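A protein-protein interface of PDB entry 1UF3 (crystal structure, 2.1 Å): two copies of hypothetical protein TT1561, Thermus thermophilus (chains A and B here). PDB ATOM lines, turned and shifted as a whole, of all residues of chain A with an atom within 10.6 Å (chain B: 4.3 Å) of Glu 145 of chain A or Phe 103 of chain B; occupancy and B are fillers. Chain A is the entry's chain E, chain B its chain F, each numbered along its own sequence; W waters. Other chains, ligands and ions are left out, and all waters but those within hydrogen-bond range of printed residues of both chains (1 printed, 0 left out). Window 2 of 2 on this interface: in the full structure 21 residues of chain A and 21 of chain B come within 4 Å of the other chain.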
ATOM      1  N   PHE A 101      12.211  29.039   0.390  1.00  0.00           N
ATOM      2  CA  PHE A 101      11.640  28.152  -0.619  1.00  0.00           C
ATOM      3  C   PHE A 101      10.187  28.467  -0.863  1.00  0.00           C
ATOM      4  O   PHE A 101       9.577  29.254  -0.127  1.00  0.00           O
ATOM      5  CB  PHE A 101      11.735  26.702  -0.139  1.00  0.00           C
ATOM      6  CG  PHE A 101      10.801  26.392   1.005  1.00  0.00           C
ATOM      7  CD1 PHE A 101       9.524  25.880   0.762  1.00  0.00           C
ATOM      8  CD2 PHE A 101      11.158  26.721   2.316  1.00  0.00           C
ATOM      9  CE1 PHE A 101       8.611  25.706   1.793  1.00  0.00           C
ATOM     10  CE2 PHE A 101      10.249  26.556   3.372  1.00  0.00           C
ATOM     11  CZ  PHE A 101       8.972  26.051   3.117  1.00  0.00           C
ATOM     12  N   PHE A 103       6.594  26.495  -3.273  1.00  0.00           N
ATOM     13  CA  PHE A 103       6.153  25.399  -4.120  1.00  0.00           C
ATOM     14  C   PHE A 103       5.440  25.921  -5.365  1.00  0.00           C
ATOM     15  O   PHE A 103       4.623  26.832  -5.285  1.00  0.00           O
ATOM     16  CB  PHE A 103       5.189  24.475  -3.368  1.00  0.00           C
ATOM     17  CG  PHE A 103       5.829  23.643  -2.290  1.00  0.00           C
ATOM     18  CD1 PHE A 103       5.631  23.950  -0.953  1.00  0.00           C
ATOM     19  CD2 PHE A 103       6.597  22.539  -2.607  1.00  0.00           C
ATOM     20  CE1 PHE A 103       6.186  23.164   0.052  1.00  0.00           C
ATOM     21  CE2 PHE A 103       7.156  21.747  -1.607  1.00  0.00           C
ATOM     22  CZ  PHE A 103       6.950  22.062  -0.274  1.00  0.00           C
ATOM     23  N   LEU A 109       9.578  22.062  -5.714  1.00  0.00           N
ATOM     24  CA  LEU A 109      10.104  22.772  -4.566  1.00  0.00           C
ATOM     25  C   LEU A 109      11.226  23.674  -5.088  1.00  0.00           C
ATOM     26  O   LEU A 109      12.294  23.187  -5.495  1.00  0.00           O
ATOM     27  CB  LEU A 109      10.635  21.754  -3.554  1.00  0.00           C
ATOM     28  CG  LEU A 109      11.319  22.250  -2.281  1.00  0.00           C
ATOM     29  CD1 LEU A 109      10.426  23.271  -1.560  1.00  0.00           C
ATOM     30  CD2 LEU A 109      11.632  21.042  -1.385  1.00  0.00           C
ATOM     31  N   TYR A 138      23.996  25.293   4.773  1.00  0.00           N
ATOM     32  CA  TYR A 138      23.092  25.370   5.913  1.00  0.00           C
ATOM     33  C   TYR A 138      21.730  25.819   5.449  1.00  0.00           C
ATOM     34  O   TYR A 138      20.720  25.323   5.915  1.00  0.00           O
ATOM     35  CB  TYR A 138      23.627  26.339   6.980  1.00  0.00           C
ATOM     36  CG  TYR A 138      22.870  26.279   8.300  1.00  0.00           C
ATOM     37  CD1 TYR A 138      23.045  25.215   9.171  1.00  0.00           C
ATOM     38  CD2 TYR A 138      21.986  27.287   8.670  1.00  0.00           C
ATOM     39  CE1 TYR A 138      22.375  25.144  10.382  1.00  0.00           C
ATOM     40  CE2 TYR A 138      21.291  27.224   9.907  1.00  0.00           C
ATOM     41  CZ  TYR A 138      21.505  26.143  10.746  1.00  0.00           C
ATOM     42  OH  TYR A 138      20.875  26.057  11.959  1.00  0.00           O
ATOM     43  N   ARG A 139      21.679  26.738   4.498  1.00  0.00           N
ATOM     44  CA  ARG A 139      20.383  27.191   4.042  1.00  0.00           C
ATOM     45  C   ARG A 139      19.575  26.075   3.386  1.00  0.00           C
ATOM     46  O   ARG A 139      18.379  25.966   3.618  1.00  0.00           O
ATOM     47  CB  ARG A 139      20.503  28.348   3.035  1.00  0.00           C
ATOM     48  CG  ARG A 139      21.283  29.575   3.490  1.00  0.00           C
ATOM     49  CD  ARG A 139      20.778  30.145   4.813  1.00  0.00           C
ATOM     50  NE  ARG A 139      21.431  31.411   5.104  1.00  0.00           N
ATOM     51  CZ  ARG A 139      21.367  32.039   6.275  1.00  0.00           C
ATOM     52  NH1 ARG A 139      20.674  31.519   7.293  1.00  0.00           N
ATOM     53  NH2 ARG A 139      21.996  33.191   6.424  1.00  0.00           N
ATOM     54  N   LEU A 140      20.215  25.250   2.558  1.00  0.00           N
ATOM     55  CA  LEU A 140      19.477  24.198   1.864  1.00  0.00           C
ATOM     56  C   LEU A 140      19.188  22.953   2.694  1.00  0.00           C
ATOM     57  O   LEU A 140      18.340  22.139   2.312  1.00  0.00           O
ATOM     58  CB  LEU A 140      20.213  23.787   0.580  1.00  0.00           C
ATOM     59  CG  LEU A 140      20.489  24.939  -0.388  1.00  0.00           C
ATOM     60  CD1 LEU A 140      21.430  24.449  -1.477  1.00  0.00           C
ATOM     61  CD2 LEU A 140      19.181  25.471  -0.978  1.00  0.00           C
ATOM     62  N   LYS A 141      19.867  22.794   3.827  1.00  0.00           N
ATOM     63  CA  LYS A 141      19.635  21.601   4.620  1.00  0.00           C
ATOM     64  C   LYS A 141      18.202  21.572   5.136  1.00  0.00           C
ATOM     65  O   LYS A 141      17.692  20.516   5.470  1.00  0.00           O
ATOM     66  CB  LYS A 141      20.640  21.491   5.783  1.00  0.00           C
ATOM     67  CG  LYS A 141      20.168  22.088   7.122  1.00  0.00           C
ATOM     68  CD  LYS A 141      21.114  21.672   8.264  1.00  0.00           C
ATOM     69  CE  LYS A 141      20.599  22.130   9.650  1.00  0.00           C
ATOM     70  NZ  LYS A 141      21.516  21.736  10.788  1.00  0.00           N
ATOM     71  N   ALA A 142      17.552  22.730   5.167  1.00  0.00           N
ATOM     72  CA  ALA A 142      16.172  22.813   5.639  1.00  0.00           C
ATOM     73  C   ALA A 142      15.251  22.012   4.729  1.00  0.00           C
ATOM     74  O   ALA A 142      14.219  21.498   5.161  1.00  0.00           O
ATOM     75  CB  ALA A 142      15.709  24.271   5.667  1.00  0.00           C
ATOM     76  N   LEU A 143      15.627  21.914   3.459  1.00  0.00           N
ATOM     77  CA  LEU A 143      14.805  21.198   2.493  1.00  0.00           C
ATOM     78  C   LEU A 143      14.665  19.696   2.786  1.00  0.00           C
ATOM     79  O   LEU A 143      13.667  19.085   2.420  1.00  0.00           O
ATOM     80  CB  LEU A 143      15.364  21.432   1.085  1.00  0.00           C
ATOM     81  CG  LEU A 143      15.629  22.907   0.718  1.00  0.00           C
ATOM     82  CD1 LEU A 143      16.316  22.994  -0.675  1.00  0.00           C
ATOM     83  CD2 LEU A 143      14.314  23.696   0.735  1.00  0.00           C
ATOM     84  N   TRP A 144      15.635  19.095   3.457  1.00  0.00           N
ATOM     85  CA  TRP A 144      15.539  17.659   3.750  1.00  0.00           C
ATOM     86  C   TRP A 144      14.273  17.298   4.530  1.00  0.00           C
ATOM     87  O   TRP A 144      13.858  16.148   4.517  1.00  0.00           O
ATOM     88  CB  TRP A 144      16.772  17.177   4.517  1.00  0.00           C
ATOM     89  CG  TRP A 144      18.042  17.249   3.719  1.00  0.00           C
ATOM     90  CD1 TRP A 144      19.230  17.834   4.092  1.00  0.00           C
ATOM     91  CD2 TRP A 144      18.260  16.699   2.419  1.00  0.00           C
ATOM     92  NE1 TRP A 144      20.168  17.673   3.101  1.00  0.00           N
ATOM     93  CE2 TRP A 144      19.599  16.982   2.062  1.00  0.00           C
ATOM     94  CE3 TRP A 144      17.454  15.993   1.518  1.00  0.00           C
ATOM     95  CZ2 TRP A 144      20.150  16.580   0.837  1.00  0.00           C
ATOM     96  CZ3 TRP A 144      18.003  15.590   0.299  1.00  0.00           C
ATOM     97  CH2 TRP A 144      19.339  15.888  -0.025  1.00  0.00           C
ATOM     98  N   GLU A 145      13.676  18.287   5.199  1.00  0.00           N
ATOM     99  CA  GLU A 145      12.446  18.105   5.982  1.00  0.00           C
ATOM    100  C   GLU A 145      11.236  17.906   5.090  1.00  0.00           C
ATOM    101  O   GLU A 145      10.226  17.353   5.529  1.00  0.00           O
ATOM    102  CB  GLU A 145      12.168  19.334   6.855  1.00  0.00           C
ATOM    103  CG  GLU A 145      13.103  19.492   8.029  1.00  0.00           C
ATOM    104  CD  GLU A 145      12.828  18.480   9.120  1.00  0.00           C
ATOM    105  OE1 GLU A 145      12.573  17.304   8.799  1.00  0.00           O
ATOM    106  OE2 GLU A 145      12.879  18.853  10.305  1.00  0.00           O
ATOM    107  N   LEU A 146      11.325  18.393   3.852  1.00  0.00           N
ATOM    108  CA  LEU A 146      10.223  18.279   2.896  1.00  0.00           C
ATOM    109  C   LEU A 146      10.450  17.027   2.056  1.00  0.00           C
ATOM    110  O   LEU A 146      11.514  16.840   1.460  1.00  0.00           O
ATOM    111  CB  LEU A 146      10.160  19.537   2.037  1.00  0.00           C
ATOM    112  CG  LEU A 146      10.064  20.777   2.933  1.00  0.00           C
ATOM    113  CD1 LEU A 146      10.068  22.052   2.071  1.00  0.00           C
ATOM    114  CD2 LEU A 146       8.797  20.678   3.803  1.00  0.00           C
ATOM    115  N   LYS A 147       9.432  16.179   2.015  1.00  0.00           N
ATOM    116  CA  LYS A 147       9.528  14.892   1.352  1.00  0.00           C
ATOM    117  C   LYS A 147       9.001  14.689  -0.057  1.00  0.00           C
ATOM    118  O   LYS A 147       7.949  15.203  -0.445  1.00  0.00           O
ATOM    119  CB  LYS A 147       8.888  13.838   2.255  1.00  0.00           C
ATOM    120  CG  LYS A 147       9.323  13.951   3.704  1.00  0.00           C
ATOM    121  CD  LYS A 147      10.824  13.730   3.840  1.00  0.00           C
ATOM    122  CE  LYS A 147      11.272  13.894   5.283  1.00  0.00           C
ATOM    123  NZ  LYS A 147      12.691  13.516   5.446  1.00  0.00           N
ATOM    124  N   ASP A 148       9.772  13.910  -0.806  1.00  0.00           N
ATOM    125  CA  ASP A 148       9.441  13.511  -2.167  1.00  0.00           C
ATOM    126  C   ASP A 148       9.051  14.600  -3.147  1.00  0.00           C
ATOM    127  O   ASP A 148       8.073  14.441  -3.883  1.00  0.00           O
ATOM    128  CB  ASP A 148       8.321  12.467  -2.119  1.00  0.00           C
ATOM    129  CG  ASP A 148       8.519  11.458  -1.001  1.00  0.00           C
ATOM    130  OD1 ASP A 148       9.611  10.845  -0.934  1.00  0.00           O
ATOM    131  OD2 ASP A 148       7.579  11.285  -0.184  1.00  0.00           O
ATOM    132  N   TYR A 149       9.792  15.703  -3.162  1.00  0.00           N
ATOM    133  CA  TYR A 149       9.512  16.789  -4.106  1.00  0.00           C
ATOM    134  C   TYR A 149      10.686  16.969  -5.044  1.00  0.00           C
ATOM    135  O   TYR A 149      11.825  16.864  -4.622  1.00  0.00           O
ATOM    136  CB  TYR A 149       9.318  18.143  -3.400  1.00  0.00           C
ATOM    137  CG  TYR A 149       8.067  18.268  -2.569  1.00  0.00           C
ATOM    138  CD1 TYR A 149       8.111  18.116  -1.190  1.00  0.00           C
ATOM    139  CD2 TYR A 149       6.843  18.559  -3.164  1.00  0.00           C
ATOM    140  CE1 TYR A 149       6.959  18.252  -0.410  1.00  0.00           C
ATOM    141  CE2 TYR A 149       5.687  18.705  -2.401  1.00  0.00           C
ATOM    142  CZ  TYR A 149       5.755  18.549  -1.023  1.00  0.00           C
ATOM    143  OH  TYR A 149       4.620  18.689  -0.263  1.00  0.00           O
ATOM    144  N   LYS A 151      13.258  19.138  -7.020  1.00  0.00           N
ATOM    145  CA  LYS A 151      13.746  20.487  -6.748  1.00  0.00           C
ATOM    146  C   LYS A 151      14.279  21.324  -7.909  1.00  0.00           C
ATOM    147  O   LYS A 151      14.814  20.800  -8.889  1.00  0.00           O
ATOM    148  CB  LYS A 151      14.848  20.410  -5.683  1.00  0.00           C
ATOM    149  CG  LYS A 151      14.402  19.835  -4.350  1.00  0.00           C
ATOM    150  CD  LYS A 151      15.581  19.228  -3.580  1.00  0.00           C
ATOM    151  CE  LYS A 151      15.132  18.703  -2.224  1.00  0.00           C
ATOM    152  NZ  LYS A 151      16.236  18.008  -1.481  1.00  0.00           N
ATOM    153  N   HIS A 179      21.568  17.316  -3.129  1.00  0.00           N
ATOM    154  CA  HIS A 179      20.122  17.421  -3.278  1.00  0.00           C
ATOM    155  C   HIS A 179      19.552  16.883  -4.578  1.00  0.00           C
ATOM    156  O   HIS A 179      18.337  16.704  -4.692  1.00  0.00           O
ATOM    157  CB  HIS A 179      19.702  18.884  -3.148  1.00  0.00           C
ATOM    158  CG  HIS A 179      19.898  19.444  -1.777  1.00  0.00           C
ATOM    159  ND1 HIS A 179      18.917  19.393  -0.807  1.00  0.00           N
ATOM    160  CD2 HIS A 179      20.980  20.016  -1.193  1.00  0.00           C
ATOM    161  CE1 HIS A 179      19.390  19.904   0.316  1.00  0.00           C
ATOM    162  NE2 HIS A 179      20.639  20.287   0.108  1.00  0.00           N
ATOM    163  N   PHE B 101      12.760  26.455   9.904  1.00  0.00           N
ATOM    164  CA  PHE B 101      11.836  25.554  10.599  1.00  0.00           C
ATOM    165  C   PHE B 101      12.337  24.125  10.656  1.00  0.00           C
ATOM    166  O   PHE B 101      13.324  23.759  10.001  1.00  0.00           O
ATOM    167  CB  PHE B 101      10.494  25.550   9.842  1.00  0.00           C
ATOM    168  CG  PHE B 101      10.584  24.864   8.489  1.00  0.00           C
ATOM    169  CD1 PHE B 101      10.311  23.493   8.360  1.00  0.00           C
ATOM    170  CD2 PHE B 101      11.114  25.545   7.389  1.00  0.00           C
ATOM    171  CE1 PHE B 101      10.587  22.808   7.147  1.00  0.00           C
ATOM    172  CE2 PHE B 101      11.392  24.873   6.175  1.00  0.00           C
ATOM    173  CZ  PHE B 101      11.131  23.505   6.061  1.00  0.00           C
ATOM    174  N   THR B 102      11.653  23.321  11.462  1.00  0.00           N
ATOM    175  CA  THR B 102      11.954  21.906  11.558  1.00  0.00           C
ATOM    176  C   THR B 102      10.659  21.228  12.038  1.00  0.00           C
ATOM    177  O   THR B 102       9.673  21.910  12.366  1.00  0.00           O
ATOM    178  CB  THR B 102      13.106  21.591  12.534  1.00  0.00           C
ATOM    179  OG1 THR B 102      13.492  20.218  12.364  1.00  0.00           O
ATOM    180  CG2 THR B 102      12.674  21.784  13.975  1.00  0.00           C
ATOM    181  N   PHE B 103      10.652  19.906  12.070  1.00  0.00           N
ATOM    182  CA  PHE B 103       9.447  19.221  12.514  1.00  0.00           C
ATOM    183  C   PHE B 103       9.742  18.389  13.721  1.00  0.00           C
ATOM    184  O   PHE B 103      10.801  17.777  13.829  1.00  0.00           O
ATOM    185  CB  PHE B 103       8.872  18.291  11.428  1.00  0.00           C
ATOM    186  CG  PHE B 103       8.322  19.009  10.240  1.00  0.00           C
ATOM    187  CD1 PHE B 103       9.078  19.133   9.076  1.00  0.00           C
ATOM    188  CD2 PHE B 103       7.042  19.540  10.276  1.00  0.00           C
ATOM    189  CE1 PHE B 103       8.565  19.772   7.958  1.00  0.00           C
ATOM    190  CE2 PHE B 103       6.511  20.187   9.162  1.00  0.00           C
ATOM    191  CZ  PHE B 103       7.272  20.304   7.994  1.00  0.00           C
ATOM    192  N   TRP B 104       8.799  18.393  14.653  1.00  0.00           N
ATOM    193  CA  TRP B 104       8.943  17.560  15.819  1.00  0.00           C
ATOM    194  C   TRP B 104       7.885  16.471  15.699  1.00  0.00           C
ATOM    195  O   TRP B 104       6.900  16.628  14.957  1.00  0.00           O
ATOM    196  CB  TRP B 104       8.721  18.368  17.102  1.00  0.00           C
ATOM    197  CG  TRP B 104       9.967  19.043  17.635  1.00  0.00           C
ATOM    198  CD1 TRP B 104      11.240  18.993  17.110  1.00  0.00           C
ATOM    199  CD2 TRP B 104      10.038  19.904  18.780  1.00  0.00           C
ATOM    200  NE1 TRP B 104      12.090  19.787  17.866  1.00  0.00           N
ATOM    201  CE2 TRP B 104      11.374  20.352  18.891  1.00  0.00           C
ATOM    202  CE3 TRP B 104       9.095  20.342  19.722  1.00  0.00           C
ATOM    203  CZ2 TRP B 104      11.789  21.218  19.910  1.00  0.00           C
ATOM    204  CZ3 TRP B 104       9.506  21.208  20.733  1.00  0.00           C
ATOM    205  CH2 TRP B 104      10.839  21.635  20.818  1.00  0.00           C
ATOM    206  N   TYR B 108       4.610  18.373  14.488  1.00  0.00           N
ATOM    207  CA  TYR B 108       4.507  19.791  14.815  1.00  0.00           C
ATOM    208  C   TYR B 108       5.549  20.541  13.993  1.00  0.00           C
ATOM    209  O   TYR B 108       6.665  20.091  13.881  1.00  0.00           O
ATOM    210  CB  TYR B 108       4.819  20.065  16.292  1.00  0.00           C
ATOM    211  CG  TYR B 108       3.731  19.648  17.208  1.00  0.00           C
ATOM    212  CD1 TYR B 108       3.801  18.439  17.890  1.00  0.00           C
ATOM    213  CD2 TYR B 108       2.603  20.441  17.379  1.00  0.00           C
ATOM    214  CE1 TYR B 108       2.769  18.020  18.720  1.00  0.00           C
ATOM    215  CE2 TYR B 108       1.550  20.022  18.218  1.00  0.00           C
ATOM    216  CZ  TYR B 108       1.648  18.811  18.871  1.00  0.00           C
ATOM    217  OH  TYR B 108       0.605  18.345  19.636  1.00  0.00           O
ATOM    218  N   LEU B 109       5.157  21.673  13.424  1.00  0.00           N
ATOM    219  CA  LEU B 109       6.052  22.528  12.655  1.00  0.00           C
ATOM    220  C   LEU B 109       6.627  23.542  13.669  1.00  0.00           C
ATOM    221  O   LEU B 109       5.891  24.387  14.192  1.00  0.00           O
ATOM    222  CB  LEU B 109       5.258  23.263  11.578  1.00  0.00           C
ATOM    223  CG  LEU B 109       5.975  24.319  10.727  1.00  0.00           C
ATOM    224  CD1 LEU B 109       7.248  23.731  10.153  1.00  0.00           C
ATOM    225  CD2 LEU B 109       5.054  24.792   9.599  1.00  0.00           C
ATOM    226  N   LEU B 146       3.502  25.458   4.249  1.00  0.00           N
ATOM    227  CA  LEU B 146       3.342  24.263   5.075  1.00  0.00           C
ATOM    228  C   LEU B 146       2.205  24.535   6.056  1.00  0.00           C
ATOM    229  O   LEU B 146       2.371  24.401   7.265  1.00  0.00           O
ATOM    230  CB  LEU B 146       4.645  24.026   5.843  1.00  0.00           C
ATOM    231  CG  LEU B 146       5.952  24.080   5.034  1.00  0.00           C
ATOM    232  CD1 LEU B 146       7.158  23.995   5.962  1.00  0.00           C
ATOM    233  CD2 LEU B 146       5.973  22.916   4.007  1.00  0.00           C
ATOM    234  N   TYR B 149      -0.083  22.004   9.435  1.00  0.00           N
ATOM    235  CA  TYR B 149       0.586  21.467  10.620  1.00  0.00           C
ATOM    236  C   TYR B 149       0.303  22.337  11.834  1.00  0.00           C
ATOM    237  O   TYR B 149       0.178  23.544  11.715  1.00  0.00           O
ATOM    238  CB  TYR B 149       2.111  21.470  10.467  1.00  0.00           C
ATOM    239  CG  TYR B 149       2.671  20.616   9.369  1.00  0.00           C
ATOM    240  CD1 TYR B 149       2.886  21.138   8.092  1.00  0.00           C
ATOM    241  CD2 TYR B 149       3.000  19.288   9.611  1.00  0.00           C
ATOM    242  CE1 TYR B 149       3.421  20.350   7.075  1.00  0.00           C
ATOM    243  CE2 TYR B 149       3.533  18.492   8.619  1.00  0.00           C
ATOM    244  CZ  TYR B 149       3.739  19.027   7.347  1.00  0.00           C
ATOM    245  OH  TYR B 149       4.239  18.213   6.370  1.00  0.00           O
HETATM  246  O   HOH W   1      14.163  22.259   8.034  1.00  0.00           O
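Of the 8 printed residues of chain B, 4 touch a printed residue of chain A. Of the 17 printed residues of chain A, 5 touch a printed residue of chain B. Among the printed residues, no Asp or Glu carboxylate lies within 4 Å of a Lys or Arg side-chain nitrogen of the other chain.
Of the printed residues of chain B, Phe 103 of chain A touches Leu 146. Tyr 138 of chain A touches none of the printed residues of chain B. Glu 145 of chain A touches just these residues of chain B: Phe 101, Thr 102 and Phe 103. Printed residues of chain B within 4 Å of Leu 146 of chain A: Leu 146. Of the printed residues of chain A, Phe 101 of chain B touches Phe 101 (3.5 Å), Ala 142 (3.8 Å) and Glu 145 (3.8 Å). Of chain A, only Glu 145 (2.5 Å) comes within 4 Å of Thr 102 of chain B. Phe 103 of chain B touches just one residue of chain A: Glu 145.
The side-chain hydroxyl (OG1) of Thr 102 of chain B sits at hydrogen-bond distance from the side-chain carboxylate (OE2) of Glu 145 of chain A (2.5 Å). The side-chain carboxylate (OE2) of Glu 145 of chain A sits at hydrogen-bond distance from the backbone NH (N) of Phe 103 of chain B (3.0 Å).
Phe 101 of chain B touches Phe 101 of chain A (CE2 to CE2, 3.5 Å). Leu 146 of chain B touches Phe 101 of chain A. CE1 of Phe 103 of chain A touches CD2 of Leu 146 of chain B (3.97 Å). O of Ala 142 of chain A touches CZ of Phe 101 of chain B (3.8 Å). Phe 101 of chain B touches Glu 145 of chain A (CE1 to CB, 3.8 Å). CD2 of Leu 146 of chain B touches CD2 of Leu 146 of chain A, at 3.6 Å.
Water W1 lies within hydrogen-bond range of O of Phe 101 of chain B (2.6 Å) and O of Ala 142 of chain A (3.0 Å).
Phe 101 of chain A touches its own counterpart, Phe 101 of chain B. Phe 101 of chain A touches Leu 146 of chain B, but with the chains exchanged Leu 146 of chain A does not touch Phe 101 of chain B (4.3 Å). Phe 103 of chain A touches Leu 146 of chain B, but with the chains exchanged Leu 146 of chain A does not touch Phe 103 of chain B (4.3 Å). Leu 146 of chain B touches its own counterpart, Leu 146 of chain A. 5 positions are printed for both chains. Of the 8 pairs that touch across the chains among the printed residues, 2 have their exchanged pair printed and touching as well.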
